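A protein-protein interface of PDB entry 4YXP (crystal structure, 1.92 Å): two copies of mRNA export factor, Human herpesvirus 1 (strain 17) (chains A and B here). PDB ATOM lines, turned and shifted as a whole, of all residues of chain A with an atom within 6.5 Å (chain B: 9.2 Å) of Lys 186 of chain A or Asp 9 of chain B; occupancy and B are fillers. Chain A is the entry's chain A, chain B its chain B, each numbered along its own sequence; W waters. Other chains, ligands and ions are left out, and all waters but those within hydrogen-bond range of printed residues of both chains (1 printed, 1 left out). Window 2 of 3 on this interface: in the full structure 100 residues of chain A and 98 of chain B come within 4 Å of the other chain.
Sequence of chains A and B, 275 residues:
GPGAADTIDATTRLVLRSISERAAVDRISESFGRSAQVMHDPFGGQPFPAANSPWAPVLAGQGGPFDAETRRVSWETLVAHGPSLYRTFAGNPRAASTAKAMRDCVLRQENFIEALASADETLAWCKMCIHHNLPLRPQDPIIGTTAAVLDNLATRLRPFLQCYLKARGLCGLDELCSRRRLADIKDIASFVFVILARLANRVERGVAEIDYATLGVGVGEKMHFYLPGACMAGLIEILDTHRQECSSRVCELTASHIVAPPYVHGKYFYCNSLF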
ATOM      1  N   ARG A 168     -16.306  26.400   1.472  1.00  0.00           N
ATOM      2  CA  ARG A 168     -16.086  25.337   0.490  1.00  0.00           C
ATOM      3  C   ARG A 168     -16.915  25.549  -0.774  1.00  0.00           C
ATOM      4  O   ARG A 168     -16.699  24.879  -1.779  1.00  0.00           O
ATOM      5  CB  ARG A 168     -16.432  23.965   1.084  1.00  0.00           C
ATOM      6  CG  ARG A 168     -15.571  23.516   2.256  1.00  0.00           C
ATOM      7  CD  ARG A 168     -14.238  22.937   1.801  1.00  0.00           C
ATOM      8  NE  ARG A 168     -13.307  23.970   1.358  1.00  0.00           N
ATOM      9  CZ  ARG A 168     -12.670  24.803   2.178  1.00  0.00           C
ATOM     10  NH1 ARG A 168     -12.870  24.733   3.488  1.00  0.00           N
ATOM     11  NH2 ARG A 168     -11.837  25.712   1.686  1.00  0.00           N
ATOM     12  N   LEU A 170     -20.207  24.944  -0.853  1.00  0.00           N
ATOM     13  CA  LEU A 170     -21.127  23.807  -0.884  1.00  0.00           C
ATOM     14  C   LEU A 170     -22.508  24.162  -0.346  1.00  0.00           C
ATOM     15  O   LEU A 170     -22.707  25.228   0.237  1.00  0.00           O
ATOM     16  CB  LEU A 170     -20.560  22.640  -0.074  1.00  0.00           C
ATOM     17  CG  LEU A 170     -19.140  22.195  -0.416  1.00  0.00           C
ATOM     18  CD1 LEU A 170     -18.730  21.040   0.485  1.00  0.00           C
ATOM     19  CD2 LEU A 170     -19.022  21.808  -1.884  1.00  0.00           C
ATOM     20  N   LEU A 182     -25.271  11.767  -3.662  1.00  0.00           N
ATOM     21  CA  LEU A 182     -23.852  11.435  -3.656  1.00  0.00           C
ATOM     22  C   LEU A 182     -23.057  12.519  -4.382  1.00  0.00           C
ATOM     23  O   LEU A 182     -21.924  12.815  -4.016  1.00  0.00           O
ATOM     24  CB  LEU A 182     -23.606  10.074  -4.306  1.00  0.00           C
ATOM     25  CG  LEU A 182     -24.223   8.866  -3.595  1.00  0.00           C
ATOM     26  CD1 LEU A 182     -23.975   7.598  -4.399  1.00  0.00           C
ATOM     27  CD2 LEU A 182     -23.679   8.721  -2.179  1.00  0.00           C
ATOM     28  N   ALA A 183     -23.669  13.114  -5.400  1.00  0.00           N
ATOM     29  CA  ALA A 183     -23.008  14.130  -6.211  1.00  0.00           C
ATOM     30  C   ALA A 183     -22.697  15.397  -5.410  1.00  0.00           C
ATOM     31  O   ALA A 183     -21.872  16.204  -5.827  1.00  0.00           O
ATOM     32  CB  ALA A 183     -23.864  14.473  -7.420  1.00  0.00           C
ATOM     33  N   ASP A 184     -23.353  15.568  -4.266  1.00  0.00           N
ATOM     34  CA  ASP A 184     -23.121  16.736  -3.418  1.00  0.00           C
ATOM     35  C   ASP A 184     -21.903  16.569  -2.505  1.00  0.00           C
ATOM     36  O   ASP A 184     -21.464  17.529  -1.872  1.00  0.00           O
ATOM     37  CB  ASP A 184     -24.356  17.031  -2.558  1.00  0.00           C
ATOM     38  CG  ASP A 184     -25.494  17.652  -3.350  1.00  0.00           C
ATOM     39  OD1 ASP A 184     -25.253  18.146  -4.471  1.00  0.00           O
ATOM     40  OD2 ASP A 184     -26.633  17.656  -2.836  1.00  0.00           O
ATOM     41  N   ILE A 185     -21.362  15.359  -2.430  1.00  0.00           N
ATOM     42  CA  ILE A 185     -20.226  15.092  -1.550  1.00  0.00           C
ATOM     43  C   ILE A 185     -18.933  15.620  -2.169  1.00  0.00           C
ATOM     44  O   ILE A 185     -18.492  15.141  -3.215  1.00  0.00           O
ATOM     45  CB  ILE A 185     -20.117  13.586  -1.237  1.00  0.00           C
ATOM     46  CG1 ILE A 185     -21.365  13.119  -0.480  1.00  0.00           C
ATOM     47  CG2 ILE A 185     -18.860  13.292  -0.419  1.00  0.00           C
ATOM     48  CD1 ILE A 185     -21.430  11.621  -0.230  1.00  0.00           C
ATOM     49  N   LYS A 186     -18.322  16.596  -1.504  1.00  0.00           N
ATOM     50  CA  LYS A 186     -17.110  17.239  -2.009  1.00  0.00           C
ATOM     51  C   LYS A 186     -16.032  17.382  -0.936  1.00  0.00           C
ATOM     52  O   LYS A 186     -14.951  17.906  -1.204  1.00  0.00           O
ATOM     53  CB  LYS A 186     -17.444  18.618  -2.584  1.00  0.00           C
ATOM     54  CG  LYS A 186     -18.473  18.595  -3.705  1.00  0.00           C
ATOM     55  CD  LYS A 186     -17.979  17.827  -4.920  1.00  0.00           C
ATOM     56  CE  LYS A 186     -19.075  17.677  -5.961  1.00  0.00           C
ATOM     57  NZ  LYS A 186     -18.804  16.559  -6.910  1.00  0.00           N
ATOM     58  N   ASP A 187     -16.324  16.915   0.273  1.00  0.00           N
ATOM     59  CA  ASP A 187     -15.358  16.961   1.367  1.00  0.00           C
ATOM     60  C   ASP A 187     -15.788  16.002   2.473  1.00  0.00           C
ATOM     61  O   ASP A 187     -16.767  15.274   2.320  1.00  0.00           O
ATOM     62  CB  ASP A 187     -15.232  18.378   1.924  1.00  0.00           C
ATOM     63  CG  ASP A 187     -16.318  18.704   2.924  1.00  0.00           C
ATOM     64  OD1 ASP A 187     -17.508  18.593   2.566  1.00  0.00           O
ATOM     65  OD2 ASP A 187     -15.980  19.049   4.075  1.00  0.00           O
ATOM     66  N   ILE A 188     -15.068  16.009   3.591  1.00  0.00           N
ATOM     67  CA  ILE A 188     -15.346  15.066   4.667  1.00  0.00           C
ATOM     68  C   ILE A 188     -16.667  15.396   5.359  1.00  0.00           C
ATOM     69  O   ILE A 188     -17.438  14.493   5.687  1.00  0.00           O
ATOM     70  CB  ILE A 188     -14.182  15.018   5.686  1.00  0.00           C
ATOM     71  CG1 ILE A 188     -14.455  13.975   6.777  1.00  0.00           C
ATOM     72  CG2 ILE A 188     -13.944  16.386   6.322  1.00  0.00           C
ATOM     73  CD1 ILE A 188     -14.584  12.546   6.262  1.00  0.00           C
ATOM     74  N   SER A 190     -19.401  16.936   4.137  1.00  0.00           N
ATOM     75  CA  SER A 190     -20.519  16.551   3.283  1.00  0.00           C
ATOM     76  C   SER A 190     -20.603  15.026   3.152  1.00  0.00           C
ATOM     77  O   SER A 190     -21.695  14.468   3.053  1.00  0.00           O
ATOM     78  CB  SER A 190     -20.404  17.212   1.903  1.00  0.00           C
ATOM     79  OG  SER A 190     -19.144  16.980   1.297  1.00  0.00           O
ATOM     80  N   PHE A 191     -19.460  14.348   3.174  1.00  0.00           N
ATOM     81  CA  PHE A 191     -19.460  12.885   3.121  1.00  0.00           C
ATOM     82  C   PHE A 191     -20.196  12.294   4.321  1.00  0.00           C
ATOM     83  O   PHE A 191     -21.111  11.487   4.164  1.00  0.00           O
ATOM     84  CB  PHE A 191     -18.034  12.330   3.073  1.00  0.00           C
ATOM     85  CG  PHE A 191     -17.972  10.831   3.197  1.00  0.00           C
ATOM     86  CD1 PHE A 191     -18.245  10.022   2.106  1.00  0.00           C
ATOM     87  CD2 PHE A 191     -17.658  10.232   4.407  1.00  0.00           C
ATOM     88  CE1 PHE A 191     -18.199   8.645   2.217  1.00  0.00           C
ATOM     89  CE2 PHE A 191     -17.613   8.853   4.523  1.00  0.00           C
ATOM     90  CZ  PHE A 191     -17.884   8.061   3.429  1.00  0.00           C
ATOM     91  N   ALA B   5     -24.764   9.292 -13.796  1.00  0.00           N
ATOM     92  CA  ALA B   5     -25.560   8.840 -12.661  1.00  0.00           C
ATOM     93  C   ALA B   5     -24.987   9.381 -11.353  1.00  0.00           C
ATOM     94  O   ALA B   5     -23.858   9.869 -11.314  1.00  0.00           O
ATOM     95  CB  ALA B   5     -25.621   7.323 -12.626  1.00  0.00           C
ATOM     96  N   ASP B   6     -25.775   9.285 -10.285  1.00  0.00           N
ATOM     97  CA  ASP B   6     -25.378   9.802  -8.979  1.00  0.00           C
ATOM     98  C   ASP B   6     -24.222   8.988  -8.403  1.00  0.00           C
ATOM     99  O   ASP B   6     -24.337   7.776  -8.220  1.00  0.00           O
ATOM    100  CB  ASP B   6     -26.568   9.782  -8.015  1.00  0.00           C
ATOM    101  CG  ASP B   6     -26.332  10.627  -6.774  1.00  0.00           C
ATOM    102  OD1 ASP B   6     -25.740  11.724  -6.902  1.00  0.00           O
ATOM    103  OD2 ASP B   6     -26.744  10.197  -5.671  1.00  0.00           O
ATOM    104  N   THR B   7     -23.113   9.659  -8.111  1.00  0.00           N
ATOM    105  CA  THR B   7     -21.925   8.985  -7.596  1.00  0.00           C
ATOM    106  C   THR B   7     -21.019   9.961  -6.846  1.00  0.00           C
ATOM    107  O   THR B   7     -21.139  11.176  -7.007  1.00  0.00           O
ATOM    108  CB  THR B   7     -21.122   8.323  -8.739  1.00  0.00           C
ATOM    109  OG1 THR B   7     -20.101   7.481  -8.191  1.00  0.00           O
ATOM    110  CG2 THR B   7     -20.481   9.379  -9.642  1.00  0.00           C
ATOM    111  N   ILE B   8     -20.122   9.426  -6.021  1.00  0.00           N
ATOM    112  CA  ILE B   8     -19.081  10.239  -5.405  1.00  0.00           C
ATOM    113  C   ILE B   8     -17.973  10.424  -6.433  1.00  0.00           C
ATOM    114  O   ILE B   8     -17.372   9.449  -6.894  1.00  0.00           O
ATOM    115  CB  ILE B   8     -18.541   9.606  -4.107  1.00  0.00           C
ATOM    116  CG1 ILE B   8     -19.675   9.372  -3.105  1.00  0.00           C
ATOM    117  CG2 ILE B   8     -17.476  10.503  -3.486  1.00  0.00           C
ATOM    118  CD1 ILE B   8     -19.278   8.525  -1.910  1.00  0.00           C
ATOM    119  N   ASP B   9     -17.705  11.672  -6.802  1.00  0.00           N
ATOM    120  CA  ASP B   9     -16.742  11.952  -7.860  1.00  0.00           C
ATOM    121  C   ASP B   9     -15.334  11.516  -7.460  1.00  0.00           C
ATOM    122  O   ASP B   9     -15.003  11.441  -6.274  1.00  0.00           O
ATOM    123  CB  ASP B   9     -16.748  13.439  -8.217  1.00  0.00           C
ATOM    124  CG  ASP B   9     -16.083  14.295  -7.160  1.00  0.00           C
ATOM    125  OD1 ASP B   9     -14.840  14.409  -7.181  1.00  0.00           O
ATOM    126  OD2 ASP B   9     -16.803  14.857  -6.313  1.00  0.00           O
ATOM    127  N   ALA B  10     -14.513  11.240  -8.467  1.00  0.00           N
ATOM    128  CA  ALA B  10     -13.178  10.692  -8.262  1.00  0.00           C
ATOM    129  C   ALA B  10     -12.265  11.636  -7.478  1.00  0.00           C
ATOM    130  O   ALA B  10     -11.475  11.190  -6.647  1.00  0.00           O
ATOM    131  CB  ALA B  10     -12.552  10.355  -9.605  1.00  0.00           C
ATOM    132  N   THR B  11     -12.363  12.933  -7.749  1.00  0.00           N
ATOM    133  CA  THR B  11     -11.526  13.911  -7.057  1.00  0.00           C
ATOM    134  C   THR B  11     -11.780  13.847  -5.559  1.00  0.00           C
ATOM    135  O   THR B  11     -10.846  13.885  -4.757  1.00  0.00           O
ATOM    136  CB  THR B  11     -11.786  15.346  -7.561  1.00  0.00           C
ATOM    137  OG1 THR B  11     -11.450  15.435  -8.950  1.00  0.00           O
ATOM    138  CG2 THR B  11     -10.951  16.364  -6.777  1.00  0.00           C
ATOM    139  N   THR B  12     -13.049  13.747  -5.184  1.00  0.00           N
ATOM    140  CA  THR B  12     -13.423  13.718  -3.778  1.00  0.00           C
ATOM    141  C   THR B  12     -12.942  12.427  -3.117  1.00  0.00           C
ATOM    142  O   THR B  12     -12.559  12.429  -1.949  1.00  0.00           O
ATOM    143  CB  THR B  12     -14.945  13.863  -3.606  1.00  0.00           C
ATOM    144  OG1 THR B  12     -15.374  15.090  -4.213  1.00  0.00           O
ATOM    145  CG2 THR B  12     -15.329  13.878  -2.134  1.00  0.00           C
ATOM    146  N   ARG B  13     -12.945  11.326  -3.864  1.00  0.00           N
ATOM    147  CA  ARG B  13     -12.460  10.057  -3.326  1.00  0.00           C
ATOM    148  C   ARG B  13     -10.977  10.154  -2.968  1.00  0.00           C
ATOM    149  O   ARG B  13     -10.527   9.538  -2.002  1.00  0.00           O
ATOM    150  CB  ARG B  13     -12.694   8.924  -4.326  1.00  0.00           C
ATOM    151  CG  ARG B  13     -14.166   8.654  -4.591  1.00  0.00           C
ATOM    152  CD  ARG B  13     -14.381   7.450  -5.497  1.00  0.00           C
ATOM    153  NE  ARG B  13     -15.795   7.297  -5.830  1.00  0.00           N
ATOM    154  CZ  ARG B  13     -16.363   6.162  -6.228  1.00  0.00           C
ATOM    155  NH1 ARG B  13     -15.644   5.052  -6.347  1.00  0.00           N
ATOM    156  NH2 ARG B  13     -17.659   6.138  -6.502  1.00  0.00           N
ATOM    157  N   LEU B  14     -10.226  10.933  -3.742  1.00  0.00           N
ATOM    158  CA  LEU B  14      -8.822  11.196  -3.443  1.00  0.00           C
ATOM    159  C   LEU B  14      -8.691  11.950  -2.127  1.00  0.00           C
ATOM    160  O   LEU B  14      -7.864  11.613  -1.282  1.00  0.00           O
ATOM    161  CB  LEU B  14      -8.169  12.009  -4.561  1.00  0.00           C
ATOM    162  CG  LEU B  14      -7.656  11.273  -5.795  1.00  0.00           C
ATOM    163  CD1 LEU B  14      -7.316  12.283  -6.880  1.00  0.00           C
ATOM    164  CD2 LEU B  14      -6.440  10.427  -5.454  1.00  0.00           C
ATOM    165  N   VAL B  15      -9.514  12.983  -1.976  1.00  0.00           N
ATOM    166  CA  VAL B  15      -9.525  13.807  -0.773  1.00  0.00           C
ATOM    167  C   VAL B  15      -9.800  12.941   0.452  1.00  0.00           C
ATOM    168  O   VAL B  15      -9.094  13.026   1.456  1.00  0.00           O
ATOM    169  CB  VAL B  15     -10.566  14.939  -0.904  1.00  0.00           C
ATOM    170  CG1 VAL B  15     -10.666  15.754   0.384  1.00  0.00           C
ATOM    171  CG2 VAL B  15     -10.213  15.847  -2.076  1.00  0.00           C
ATOM    172  N   LEU B  16     -10.825  12.102   0.362  1.00  0.00           N
ATOM    173  CA  LEU B  16     -11.229  11.263   1.485  1.00  0.00           C
ATOM    174  C   LEU B  16     -10.137  10.275   1.900  1.00  0.00           C
ATOM    175  O   LEU B  16      -9.893  10.082   3.091  1.00  0.00           O
ATOM    176  CB  LEU B  16     -12.516  10.504   1.143  1.00  0.00           C
ATOM    177  CG  LEU B  16     -13.766  11.366   0.939  1.00  0.00           C
ATOM    178  CD1 LEU B  16     -14.937  10.509   0.482  1.00  0.00           C
ATOM    179  CD2 LEU B  16     -14.134  12.127   2.204  1.00  0.00           C
HETATM  180  O   HOH W   1     -13.606  17.336  -3.906  1.00  0.00           O
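OD2 of Asp 6 of chain B sits at hydrogen-bond distance from N of Leu 182 of chain A, 2.9 Å away. The backbone carbonyl oxygen (O) of Leu 182 of chain A lies close to the backbone carbonyl oxygen (O) of Thr 7 of chain B (3.5 Å). OD1 of Asp 6 of chain B is in hydrogen-bond range of N of Ala 183 of chain A, at 2.9 Å. The backbone carbonyl oxygen (O) of Ile 185 of chain A lies within hydrogen-bond range of the side-chain hydroxyl (OG1) of Thr 12 of chain B, at 3.3 Å. The side-chain amino group (NZ) of Lys 186 of chain A lies within salt-bridge range of the side-chain carboxylate (OD2) of Asp 9 of chain B, 2.7 Å away.
Water W1 bridges the side-chain hydroxyl (OG1) of Thr 12 of chain B (2.9 Å) and the backbone carbonyl oxygen (O) of Lys 186 of chain A (3.1 Å).
O of Ile 8 of chain B lies within hydrogen-bond range of NE of Arg 13 of chain B (2.9 Å). N of Thr 11 of chain B is in hydrogen-bond range of OD1 of Asp 9 of chain B, at 2.9 Å. NH2 of Arg 13 of chain B is in hydrogen-bond range of OG1 of Thr 7 of chain B (3.3 Å). O of Ala 183 of chain A sits close to NZ of Lys 186 of chain A. The side-chain hydroxyl of Thr 12 of chain B lies within hydrogen-bond range of the side-chain carboxylate of Asp 9 of chain B (2.6 Å). OG of Ser 190 of chain A lies within hydrogen-bond range of N of Lys 186 of chain A (2.9 Å).
Of the 12 printed residues of chain B, 6 touch a printed residue of chain A. Printed residues of chain B that touch a printed residue of chain A: Asp 6, Thr 7, Ile 8, Asp 9, Thr 12 and Leu 16. Hydrophobic or aromatic side chains of chain B within 4 Å of the printed part of chain A: Leu 16. Of the 11 printed residues of chain A, 5 touch a printed residue of chain B. Printed residues of chain A that touch a printed residue of chain B: Leu 182, Ala 183, Ile 185, Lys 186 and Phe 191. Among the printed residues, 10 pairs touch across the chains. Among the printed residues, Asp or Glu carboxylates within 4 Å of a Lys or Arg side-chain nitrogen of the other chain: Lys 186 of chain A with Asp 9 of chain B (2.7 Å).
No position is printed for both chains. Of the 10 pairs that touch across the chains among the printed residues, none has its exchanged pair printed and touching as well.
Leu 182 of chain A touches Ile 8 of chain B. Ala 183 of chain A touches Thr 7 of chain B. Ile 185 of chain A touches Asp 9 of chain B (O to OD2, 3.5 Å). Lys 186 of chain A touches Thr 12 of chain B (CA to OG1, 3.5 Å). CD1 of Phe 191 of chain A touches CD1 of Leu 16 of chain B (3.7 Å).
Of chain B, only Asp 9 (2.7 Å) and Thr 12 (3.5 Å) come within 4 Å of Lys 186 of chain A. Printed residues of chain B within 4 Å of Ala 183 of chain A: Asp 6 (2.9 Å) and Thr 7 (3.6 Å). Printed residues of chain A within 4 Å of Asp 6 of chain B: Leu 182 (2.9 Å) and Ala 183 (2.9 Å). Printed residues of chain B within 4 Å of Ile 185 of chain A: Asp 9 (3.5 Å) and Thr 12 (3.3 Å). Of the printed residues of chain B, Leu 182 of chain A touches Asp 6 (2.9 Å), Thr 7 (3.5 Å) and Ile 8 (3.9 Å). Of the printed residues of chain A, Leu 16 of chain B touches Phe 191 (3.7 Å). The nearest residue of chain B that does not touch Lys 186 of chain A is Val 15 of chain B (5.1 Å).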
